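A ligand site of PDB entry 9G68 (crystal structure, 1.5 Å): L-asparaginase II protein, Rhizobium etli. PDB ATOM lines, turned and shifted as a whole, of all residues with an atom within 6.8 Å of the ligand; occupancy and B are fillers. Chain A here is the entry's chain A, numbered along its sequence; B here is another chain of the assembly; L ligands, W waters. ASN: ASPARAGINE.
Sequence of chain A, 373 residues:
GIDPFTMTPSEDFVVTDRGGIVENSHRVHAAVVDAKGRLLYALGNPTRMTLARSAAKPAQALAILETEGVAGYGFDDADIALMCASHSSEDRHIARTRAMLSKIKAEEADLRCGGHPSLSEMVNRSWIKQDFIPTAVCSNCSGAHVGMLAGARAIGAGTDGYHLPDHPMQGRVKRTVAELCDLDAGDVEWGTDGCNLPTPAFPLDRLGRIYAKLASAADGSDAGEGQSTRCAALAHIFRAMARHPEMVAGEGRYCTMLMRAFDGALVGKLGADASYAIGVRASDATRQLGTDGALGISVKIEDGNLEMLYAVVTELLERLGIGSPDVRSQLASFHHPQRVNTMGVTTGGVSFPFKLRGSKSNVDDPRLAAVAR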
ATOM      1  N   ALA A  52      36.052 -21.955 -22.450  1.00  0.00           N
ATOM      2  CA  ALA A  52      35.909 -22.844 -23.592  1.00  0.00           C
ATOM      3  C   ALA A  52      34.717 -23.768 -23.429  1.00  0.00           C
ATOM      4  O   ALA A  52      34.182 -24.243 -24.438  1.00  0.00           O
ATOM      5  CB  ALA A  52      37.183 -23.664 -23.816  1.00  0.00           C
ATOM      6  N   ARG A  53      34.305 -24.025 -22.175  1.00  0.00           N
ATOM      7  CA  ARG A  53      33.196 -24.914 -21.879  1.00  0.00           C
ATOM      8  C   ARG A  53      33.433 -26.229 -22.625  1.00  0.00           C
ATOM      9  O   ARG A  53      34.578 -26.719 -22.632  1.00  0.00           O
ATOM     10  CB  ARG A  53      31.863 -24.245 -22.247  1.00  0.00           C
ATOM     11  CG  ARG A  53      31.620 -22.841 -21.614  1.00  0.00           C
ATOM     12  CD  ARG A  53      31.536 -22.934 -20.066  1.00  0.00           C
ATOM     13  NE  ARG A  53      30.297 -23.622 -19.686  1.00  0.00           N
ATOM     14  CZ  ARG A  53      29.096 -23.101 -19.832  1.00  0.00           C
ATOM     15  NH1 ARG A  53      28.912 -21.866 -20.289  1.00  0.00           N
ATOM     16  NH2 ARG A  53      28.026 -23.846 -19.572  1.00  0.00           N
ATOM     17  N   SER A  54      32.425 -26.799 -23.282  1.00  0.00           N
ATOM     18  CA  SER A  54      32.604 -28.108 -23.900  1.00  0.00           C
ATOM     19  C   SER A  54      33.470 -28.083 -25.150  1.00  0.00           C
ATOM     20  O   SER A  54      33.804 -29.149 -25.670  1.00  0.00           O
ATOM     21  CB  SER A  54      31.255 -28.735 -24.252  1.00  0.00           C
ATOM     22  OG  SER A  54      30.653 -29.366 -23.120  1.00  0.00           O
ATOM     23  N   ALA A  55      33.858 -26.911 -25.656  1.00  0.00           N
ATOM     24  CA  ALA A  55      34.858 -26.951 -26.730  1.00  0.00           C
ATOM     25  C   ALA A  55      36.207 -27.450 -26.224  1.00  0.00           C
ATOM     26  O   ALA A  55      37.059 -27.818 -27.032  1.00  0.00           O
ATOM     27  CB  ALA A  55      34.999 -25.575 -27.387  1.00  0.00           C
ATOM     28  N   LYS A  57      36.327 -30.286 -24.554  1.00  0.00           N
ATOM     29  CA  LYS A  57      36.173 -31.736 -24.366  1.00  0.00           C
ATOM     30  C   LYS A  57      37.263 -32.564 -25.035  1.00  0.00           C
ATOM     31  O   LYS A  57      37.716 -33.532 -24.408  1.00  0.00           O
ATOM     32  CB  LYS A  57      34.789 -32.191 -24.870  1.00  0.00           C
ATOM     33  CG  LYS A  57      33.610 -31.816 -23.995  1.00  0.00           C
ATOM     34  CD  LYS A  57      33.654 -32.511 -22.649  1.00  0.00           C
ATOM     35  CE  LYS A  57      32.429 -32.155 -21.800  1.00  0.00           C
ATOM     36  NZ  LYS A  57      32.850 -31.618 -20.468  1.00  0.00           N
ATOM     37  N   ALA A  85      31.849 -35.263 -26.526  1.00  0.00           N
ATOM     38  CA  ALA A  85      30.544 -34.780 -26.992  1.00  0.00           C
ATOM     39  C   ALA A  85      29.882 -33.761 -26.060  1.00  0.00           C
ATOM     40  O   ALA A  85      30.189 -33.679 -24.869  1.00  0.00           O
ATOM     41  CB  ALA A  85      29.566 -35.943 -27.170  1.00  0.00           C
ATOM     42  N   SER A  86      28.946 -33.015 -26.649  1.00  0.00           N
ATOM     43  CA  SER A  86      27.820 -32.361 -25.945  1.00  0.00           C
ATOM     44  C   SER A  86      26.606 -32.925 -26.638  1.00  0.00           C
ATOM     45  O   SER A  86      26.041 -32.261 -27.502  1.00  0.00           O
ATOM     46  CB  SER A  86      27.811 -30.846 -26.015  1.00  0.00           C
ATOM     47  OG  SER A  86      29.004 -30.286 -25.509  1.00  0.00           O
ATOM     48  N   GLY A 114      24.719 -34.313 -13.633  1.00  0.00           N
ATOM     49  CA  GLY A 114      23.278 -34.356 -13.437  1.00  0.00           C
ATOM     50  C   GLY A 114      22.468 -34.208 -14.714  1.00  0.00           C
ATOM     51  O   GLY A 114      23.004 -33.750 -15.740  1.00  0.00           O
ATOM     52  N   HIS A 116      19.525 -32.777 -17.349  1.00  0.00           N
ATOM     53  CA  HIS A 116      19.108 -31.442 -17.740  1.00  0.00           C
ATOM     54  C   HIS A 116      18.199 -31.557 -18.973  1.00  0.00           C
ATOM     55  O   HIS A 116      18.219 -32.590 -19.661  1.00  0.00           O
ATOM     56  CB  HIS A 116      20.326 -30.581 -18.055  1.00  0.00           C
ATOM     57  CG  HIS A 116      21.213 -31.202 -19.091  1.00  0.00           C
ATOM     58  ND1 HIS A 116      20.897 -31.173 -20.436  1.00  0.00           N
ATOM     59  CD2 HIS A 116      22.351 -31.926 -18.978  1.00  0.00           C
ATOM     60  CE1 HIS A 116      21.835 -31.836 -21.108  1.00  0.00           C
ATOM     61  NE2 HIS A 116      22.725 -32.297 -20.248  1.00  0.00           N
ATOM     62  N   LEU A 119      19.634 -30.846 -25.167  1.00  0.00           N
ATOM     63  CA  LEU A 119      20.135 -29.814 -26.074  1.00  0.00           C
ATOM     64  C   LEU A 119      19.361 -29.781 -27.391  1.00  0.00           C
ATOM     65  O   LEU A 119      19.453 -28.783 -28.116  1.00  0.00           O
ATOM     66  CB  LEU A 119      21.632 -30.038 -26.329  1.00  0.00           C
ATOM     67  CG  LEU A 119      22.568 -29.793 -25.130  1.00  0.00           C
ATOM     68  CD1 LEU A 119      23.995 -30.116 -25.525  1.00  0.00           C
ATOM     69  CD2 LEU A 119      22.502 -28.340 -24.646  1.00  0.00           C
ATOM     70  N   SER A 139      23.148 -36.829 -19.105  1.00  0.00           N
ATOM     71  CA  SER A 139      23.940 -35.607 -19.234  1.00  0.00           C
ATOM     72  C   SER A 139      24.611 -35.534 -20.601  1.00  0.00           C
ATOM     73  O   SER A 139      25.156 -36.532 -21.085  1.00  0.00           O
ATOM     74  CB  SER A 139      25.002 -35.538 -18.132  1.00  0.00           C
ATOM     75  OG  SER A 139      26.007 -34.570 -18.468  1.00  0.00           O
ATOM     76  N   ASN A 140      24.571 -34.342 -21.218  1.00  0.00           N
ATOM     77  CA  ASN A 140      25.241 -34.147 -22.503  1.00  0.00           C
ATOM     78  C   ASN A 140      26.742 -34.428 -22.406  1.00  0.00           C
ATOM     79  O   ASN A 140      27.376 -34.731 -23.421  1.00  0.00           O
ATOM     80  CB  ASN A 140      24.985 -32.719 -23.017  1.00  0.00           C
ATOM     81  CG  ASN A 140      25.893 -31.682 -22.338  1.00  0.00           C
ATOM     82  OD1 ASN A 140      26.931 -31.291 -22.893  1.00  0.00           O
ATOM     83  ND2 ASN A 140      25.520 -31.248 -21.146  1.00  0.00           N
ATOM     84  N   CYS A 141      27.306 -34.383 -21.184  1.00  0.00           N
ATOM     85  CA  CYS A 141      28.707 -34.653 -20.904  1.00  0.00           C
ATOM     86  C   CYS A 141      28.945 -36.056 -20.331  1.00  0.00           C
ATOM     87  O   CYS A 141      30.029 -36.316 -19.788  1.00  0.00           O
ATOM     88  CB  CYS A 141      29.250 -33.603 -19.942  1.00  0.00           C
ATOM     89  SG  CYS A 141      29.137 -31.961 -20.648  1.00  0.00           S
ATOM     90  N   HIS A 145      32.360 -37.872 -18.461  1.00  0.00           N
ATOM     91  CA  HIS A 145      32.301 -38.344 -17.079  1.00  0.00           C
ATOM     92  C   HIS A 145      32.623 -39.825 -16.978  1.00  0.00           C
ATOM     93  O   HIS A 145      33.357 -40.239 -16.060  1.00  0.00           O
ATOM     94  CB  HIS A 145      30.927 -38.041 -16.476  1.00  0.00           C
ATOM     95  CG  HIS A 145      30.829 -36.639 -15.990  1.00  0.00           C
ATOM     96  ND1 HIS A 145      30.925 -36.294 -14.664  1.00  0.00           N
ATOM     97  CD2 HIS A 145      30.703 -35.467 -16.671  1.00  0.00           C
ATOM     98  CE1 HIS A 145      30.808 -34.981 -14.536  1.00  0.00           C
ATOM     99  NE2 HIS A 145      30.684 -34.456 -15.740  1.00  0.00           N
ATOM    100  N   ASP A 193      31.523 -26.165 -14.409  1.00  0.00           N
ATOM    101  CA  ASP A 193      30.606 -26.241 -15.534  1.00  0.00           C
ATOM    102  C   ASP A 193      29.236 -26.759 -15.108  1.00  0.00           C
ATOM    103  O   ASP A 193      29.018 -27.155 -13.955  1.00  0.00           O
ATOM    104  CB  ASP A 193      31.207 -27.132 -16.617  1.00  0.00           C
ATOM    105  CG  ASP A 193      30.893 -26.632 -18.031  1.00  0.00           C
ATOM    106  OD1 ASP A 193      29.871 -25.948 -18.197  1.00  0.00           O
ATOM    107  OD2 ASP A 193      31.673 -26.951 -18.974  1.00  0.00           O
ATOM    108  N   GLY A 194      28.297 -26.799 -16.067  1.00  0.00           N
ATOM    109  CA  GLY A 194      26.947 -27.268 -15.773  1.00  0.00           C
ATOM    110  C   GLY A 194      26.898 -28.738 -15.361  1.00  0.00           C
ATOM    111  O   GLY A 194      26.001 -29.158 -14.622  1.00  0.00           O
ATOM    112  N   CYS A 195      27.856 -29.528 -15.854  1.00  0.00           N
ATOM    113  CA  CYS A 195      27.959 -30.944 -15.534  1.00  0.00           C
ATOM    114  C   CYS A 195      28.870 -31.191 -14.335  1.00  0.00           C
ATOM    115  O   CYS A 195      29.271 -32.329 -14.086  1.00  0.00           O
ATOM    116  CB  CYS A 195      28.444 -31.725 -16.752  1.00  0.00           C
ATOM    117  SG  CYS A 195      30.157 -31.314 -17.218  1.00  0.00           S
ATOM    118  N   ASN A 196      29.234 -30.118 -13.622  1.00  0.00           N
ATOM    119  CA  ASN A 196      29.900 -30.142 -12.318  1.00  0.00           C
ATOM    120  C   ASN A 196      31.367 -30.543 -12.392  1.00  0.00           C
ATOM    121  O   ASN A 196      31.939 -30.989 -11.378  1.00  0.00           O
ATOM    122  CB  ASN A 196      29.165 -31.057 -11.327  1.00  0.00           C
ATOM    123  CG  ASN A 196      29.371 -30.639  -9.897  1.00  0.00           C
ATOM    124  OD1 ASN A 196      29.563 -29.461  -9.608  1.00  0.00           O
ATOM    125  ND2 ASN A 196      29.372 -31.600  -8.982  1.00  0.00           N
ATOM    126  N   LEU A 197      32.018 -30.381 -13.576  1.00  0.00           N
ATOM    127  CA  LEU A 197      33.469 -30.550 -13.742  1.00  0.00           C
ATOM    128  C   LEU A 197      34.175 -29.203 -13.718  1.00  0.00           C
ATOM    129  O   LEU A 197      33.592 -28.164 -14.046  1.00  0.00           O
ATOM    130  CB  LEU A 197      33.779 -31.244 -15.062  1.00  0.00           C
ATOM    131  CG  LEU A 197      33.580 -32.753 -15.116  1.00  0.00           C
ATOM    132  CD1 LEU A 197      33.740 -33.223 -16.531  1.00  0.00           C
ATOM    133  CD2 LEU A 197      34.597 -33.449 -14.174  1.00  0.00           C
ATOM    134  N   THR A 199      36.186 -26.348 -15.384  1.00  0.00           N
ATOM    135  CA  THR A 199      36.128 -25.914 -16.791  1.00  0.00           C
ATOM    136  C   THR A 199      37.045 -24.706 -17.007  1.00  0.00           C
ATOM    137  O   THR A 199      37.091 -23.815 -16.150  1.00  0.00           O
ATOM    138  CB  THR A 199      34.672 -25.600 -17.219  1.00  0.00           C
ATOM    139  OG1 THR A 199      34.591 -25.476 -18.634  1.00  0.00           O
ATOM    140  CG2 THR A 199      34.120 -24.316 -16.564  1.00  0.00           C
ATOM    141  N   LYS A 269      33.362 -28.315 -32.873  1.00  0.00           N
ATOM    142  CA  LYS A 269      32.757 -28.588 -31.585  1.00  0.00           C
ATOM    143  C   LYS A 269      32.183 -27.308 -30.979  1.00  0.00           C
ATOM    144  O   LYS A 269      32.832 -26.258 -30.975  1.00  0.00           O
ATOM    145  CB  LYS A 269      33.790 -29.205 -30.637  1.00  0.00           C
ATOM    146  CG  LYS A 269      33.262 -29.485 -29.251  1.00  0.00           C
ATOM    147  CD  LYS A 269      32.424 -30.764 -29.214  1.00  0.00           C
ATOM    148  CE  LYS A 269      31.710 -30.883 -27.860  1.00  0.00           C
ATOM    149  NZ  LYS A 269      30.589 -29.910 -27.757  1.00  0.00           N
ATOM    150  N   LEU A 270      30.966 -27.420 -30.430  1.00  0.00           N
ATOM    151  CA  LEU A 270      30.308 -26.316 -29.733  1.00  0.00           C
ATOM    152  C   LEU A 270      30.770 -26.160 -28.292  1.00  0.00           C
ATOM    153  O   LEU A 270      30.963 -27.146 -27.575  1.00  0.00           O
ATOM    154  CB  LEU A 270      28.800 -26.564 -29.742  1.00  0.00           C
ATOM    155  CG  LEU A 270      27.977 -25.659 -28.872  1.00  0.00           C
ATOM    156  CD1 LEU A 270      27.928 -24.288 -29.556  1.00  0.00           C
ATOM    157  CD2 LEU A 270      26.574 -26.268 -28.731  1.00  0.00           C
ATOM    158  N   GLY A 271      30.925 -24.911 -27.853  1.00  0.00           N
ATOM    159  CA  GLY A 271      31.030 -24.557 -26.442  1.00  0.00           C
ATOM    160  C   GLY A 271      29.771 -23.816 -26.006  1.00  0.00           C
ATOM    161  O   GLY A 271      29.330 -22.879 -26.677  1.00  0.00           O
ATOM    162  N   ALA A 272      29.199 -24.238 -24.881  1.00  0.00           N
ATOM    163  CA  ALA A 272      28.033 -23.534 -24.370  1.00  0.00           C
ATOM    164  C   ALA A 272      28.279 -22.031 -24.212  1.00  0.00           C
ATOM    165  O   ALA A 272      29.428 -21.588 -24.045  1.00  0.00           O
ATOM    166  CB  ALA A 272      27.597 -24.136 -23.037  1.00  0.00           C
ATOM    167  N   ASP A 273      27.205 -21.254 -24.247  1.00  0.00           N
ATOM    168  CA  ASP A 273      27.272 -19.799 -24.302  1.00  0.00           C
ATOM    169  C   ASP A 273      28.077 -19.336 -25.515  1.00  0.00           C
ATOM    170  O   ASP A 273      28.647 -18.235 -25.517  1.00  0.00           O
ATOM    171  CB  ASP A 273      27.777 -19.214 -22.970  1.00  0.00           C
ATOM    172  CG  ASP A 273      26.715 -19.341 -21.878  1.00  0.00           C
ATOM    173  OD1 ASP A 273      25.604 -18.802 -22.089  1.00  0.00           O
ATOM    174  OD2 ASP A 273      26.935 -20.033 -20.861  1.00  0.00           O
ATOM    175  N   ARG B  18      31.160 -16.885 -14.543  1.00  0.00           N
ATOM    176  CA  ARG B  18      31.297 -18.233 -13.984  1.00  0.00           C
ATOM    177  C   ARG B  18      32.515 -18.208 -13.063  1.00  0.00           C
ATOM    178  O   ARG B  18      33.650 -18.050 -13.516  1.00  0.00           O
ATOM    179  CB  ARG B  18      31.412 -19.256 -15.119  1.00  0.00           C
ATOM    180  CG  ARG B  18      31.402 -20.731 -14.697  1.00  0.00           C
ATOM    181  CD  ARG B  18      31.314 -21.643 -15.933  1.00  0.00           C
ATOM    182  NE  ARG B  18      30.082 -21.389 -16.681  1.00  0.00           N
ATOM    183  CZ  ARG B  18      28.935 -22.013 -16.464  1.00  0.00           C
ATOM    184  NH1 ARG B  18      28.836 -23.003 -15.583  1.00  0.00           N
ATOM    185  NH2 ARG B  18      27.846 -21.644 -17.152  1.00  0.00           N
ATOM    186  N   THR B 342      23.729 -28.769 -12.807  1.00  0.00           N
ATOM    187  CA  THR B 342      22.868 -29.934 -12.750  1.00  0.00           C
ATOM    188  C   THR B 342      23.008 -30.703 -11.445  1.00  0.00           C
ATOM    189  O   THR B 342      22.229 -31.624 -11.191  1.00  0.00           O
ATOM    190  CB  THR B 342      23.154 -30.847 -13.946  1.00  0.00           C
ATOM    191  OG1 THR B 342      24.498 -31.354 -13.865  1.00  0.00           O
ATOM    192  CG2 THR B 342      22.963 -30.065 -15.264  1.00  0.00           C
HETATM  193  N   ASN L   1      27.210 -26.448 -19.216  1.00  0.00           N
HETATM  194  CA  ASN L   1      27.595 -27.519 -20.108  1.00  0.00           C
HETATM  195  C   ASN L   1      27.667 -28.777 -19.274  1.00  0.00           C
HETATM  196  O   ASN L   1      28.577 -28.948 -18.459  1.00  0.00           O
HETATM  197  CB  ASN L   1      28.943 -27.254 -20.801  1.00  0.00           C
HETATM  198  CG  ASN L   1      28.840 -27.368 -22.327  1.00  0.00           C
HETATM  199  OD1 ASN L   1      29.458 -26.602 -23.081  1.00  0.00           O
HETATM  200  ND2 ASN L   1      28.060 -28.355 -22.796  1.00  0.00           N
HETATM  201  OXT ASN L   1      26.815 -29.637 -19.374  1.00  0.00           O
HETATM  202  O   HOH W   1      25.759 -26.744 -24.762  1.00  0.00           O
HETATM  203  O   HOH W   2      24.849 -25.058 -18.356  1.00  0.00           O
HETATM  204  O   HOH W   3      28.194 -27.629 -25.399  1.00  0.00           O
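Water W3 bridges ND2 of the ligand (2.7 Å) and OG of Ser 86 (2.8 Å).
Of the 27 residues printed, 9 come within 4 Å of the ligand.
NE of Arg 53 is in salt-bridge range of OD1 of Asp 193. NE2 of His 145 lies within hydrogen-bond range of O of Cys 195. SG of Cys 141 sits at hydrogen-bond distance from OD1 of Asn 140 (3.2 Å). The backbone NH (N) of Asn 140 is in hydrogen-bond range of a ring nitrogen (NE2) of His 116 (2.9 Å). The side-chain carboxylate (OD2) of Asp 193 sits at hydrogen-bond distance from the side-chain hydroxyl (OG1) of Thr 199 (3.3 Å). The side-chain amino group of Lys 269 lies within hydrogen-bond range of the side-chain hydroxyl of Ser 86, at 2.8 Å. The side-chain sulfur (SG) of Cys 141 sits close to the side-chain amino group (NZ) of Lys 57 (3.7 Å). The side-chain hydroxyl (OG) of Ser 54 lies close to the side-chain hydroxyl (OG) of Ser 86 (3.0 Å).
SG of Cys 195 sits at hydrogen-bond distance from O of the ligand, at 3.1 Å. The guanidinium group (NH2) of Arg 53 lies close to a nitrogen (N) of the ligand (2.8 Å). SG of Cys 141 sits at hydrogen-bond distance from OXT of the ligand, at 3.5 Å. OXT of the ligand sits at hydrogen-bond distance from ND2 of Asn 140 (2.7 Å). A nitrogen (ND2) of the ligand lies within hydrogen-bond range of the side-chain hydroxyl (OG) of Ser 54 (2.8 Å). The side-chain carboxylate (OD1) of Asp 193 lies within salt-bridge range of a nitrogen (N) of the ligand (2.9 Å). The backbone NH (N) of Ala 272 is in hydrogen-bond range of an oxygen (OD1) of the ligand. OG of Ser 86 sits at hydrogen-bond distance from ND2 of the ligand, 3.5 Å away. An oxygen (O) of the ligand lies within hydrogen-bond range of the backbone NH of Cys 195 (2.8 Å). An oxygen (OD1) of the ligand is in hydrogen-bond range of the backbone NH (N) of Ser 54, 3.0 Å away. N of Gly 194 is in hydrogen-bond range of O of the ligand (3.2 Å).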
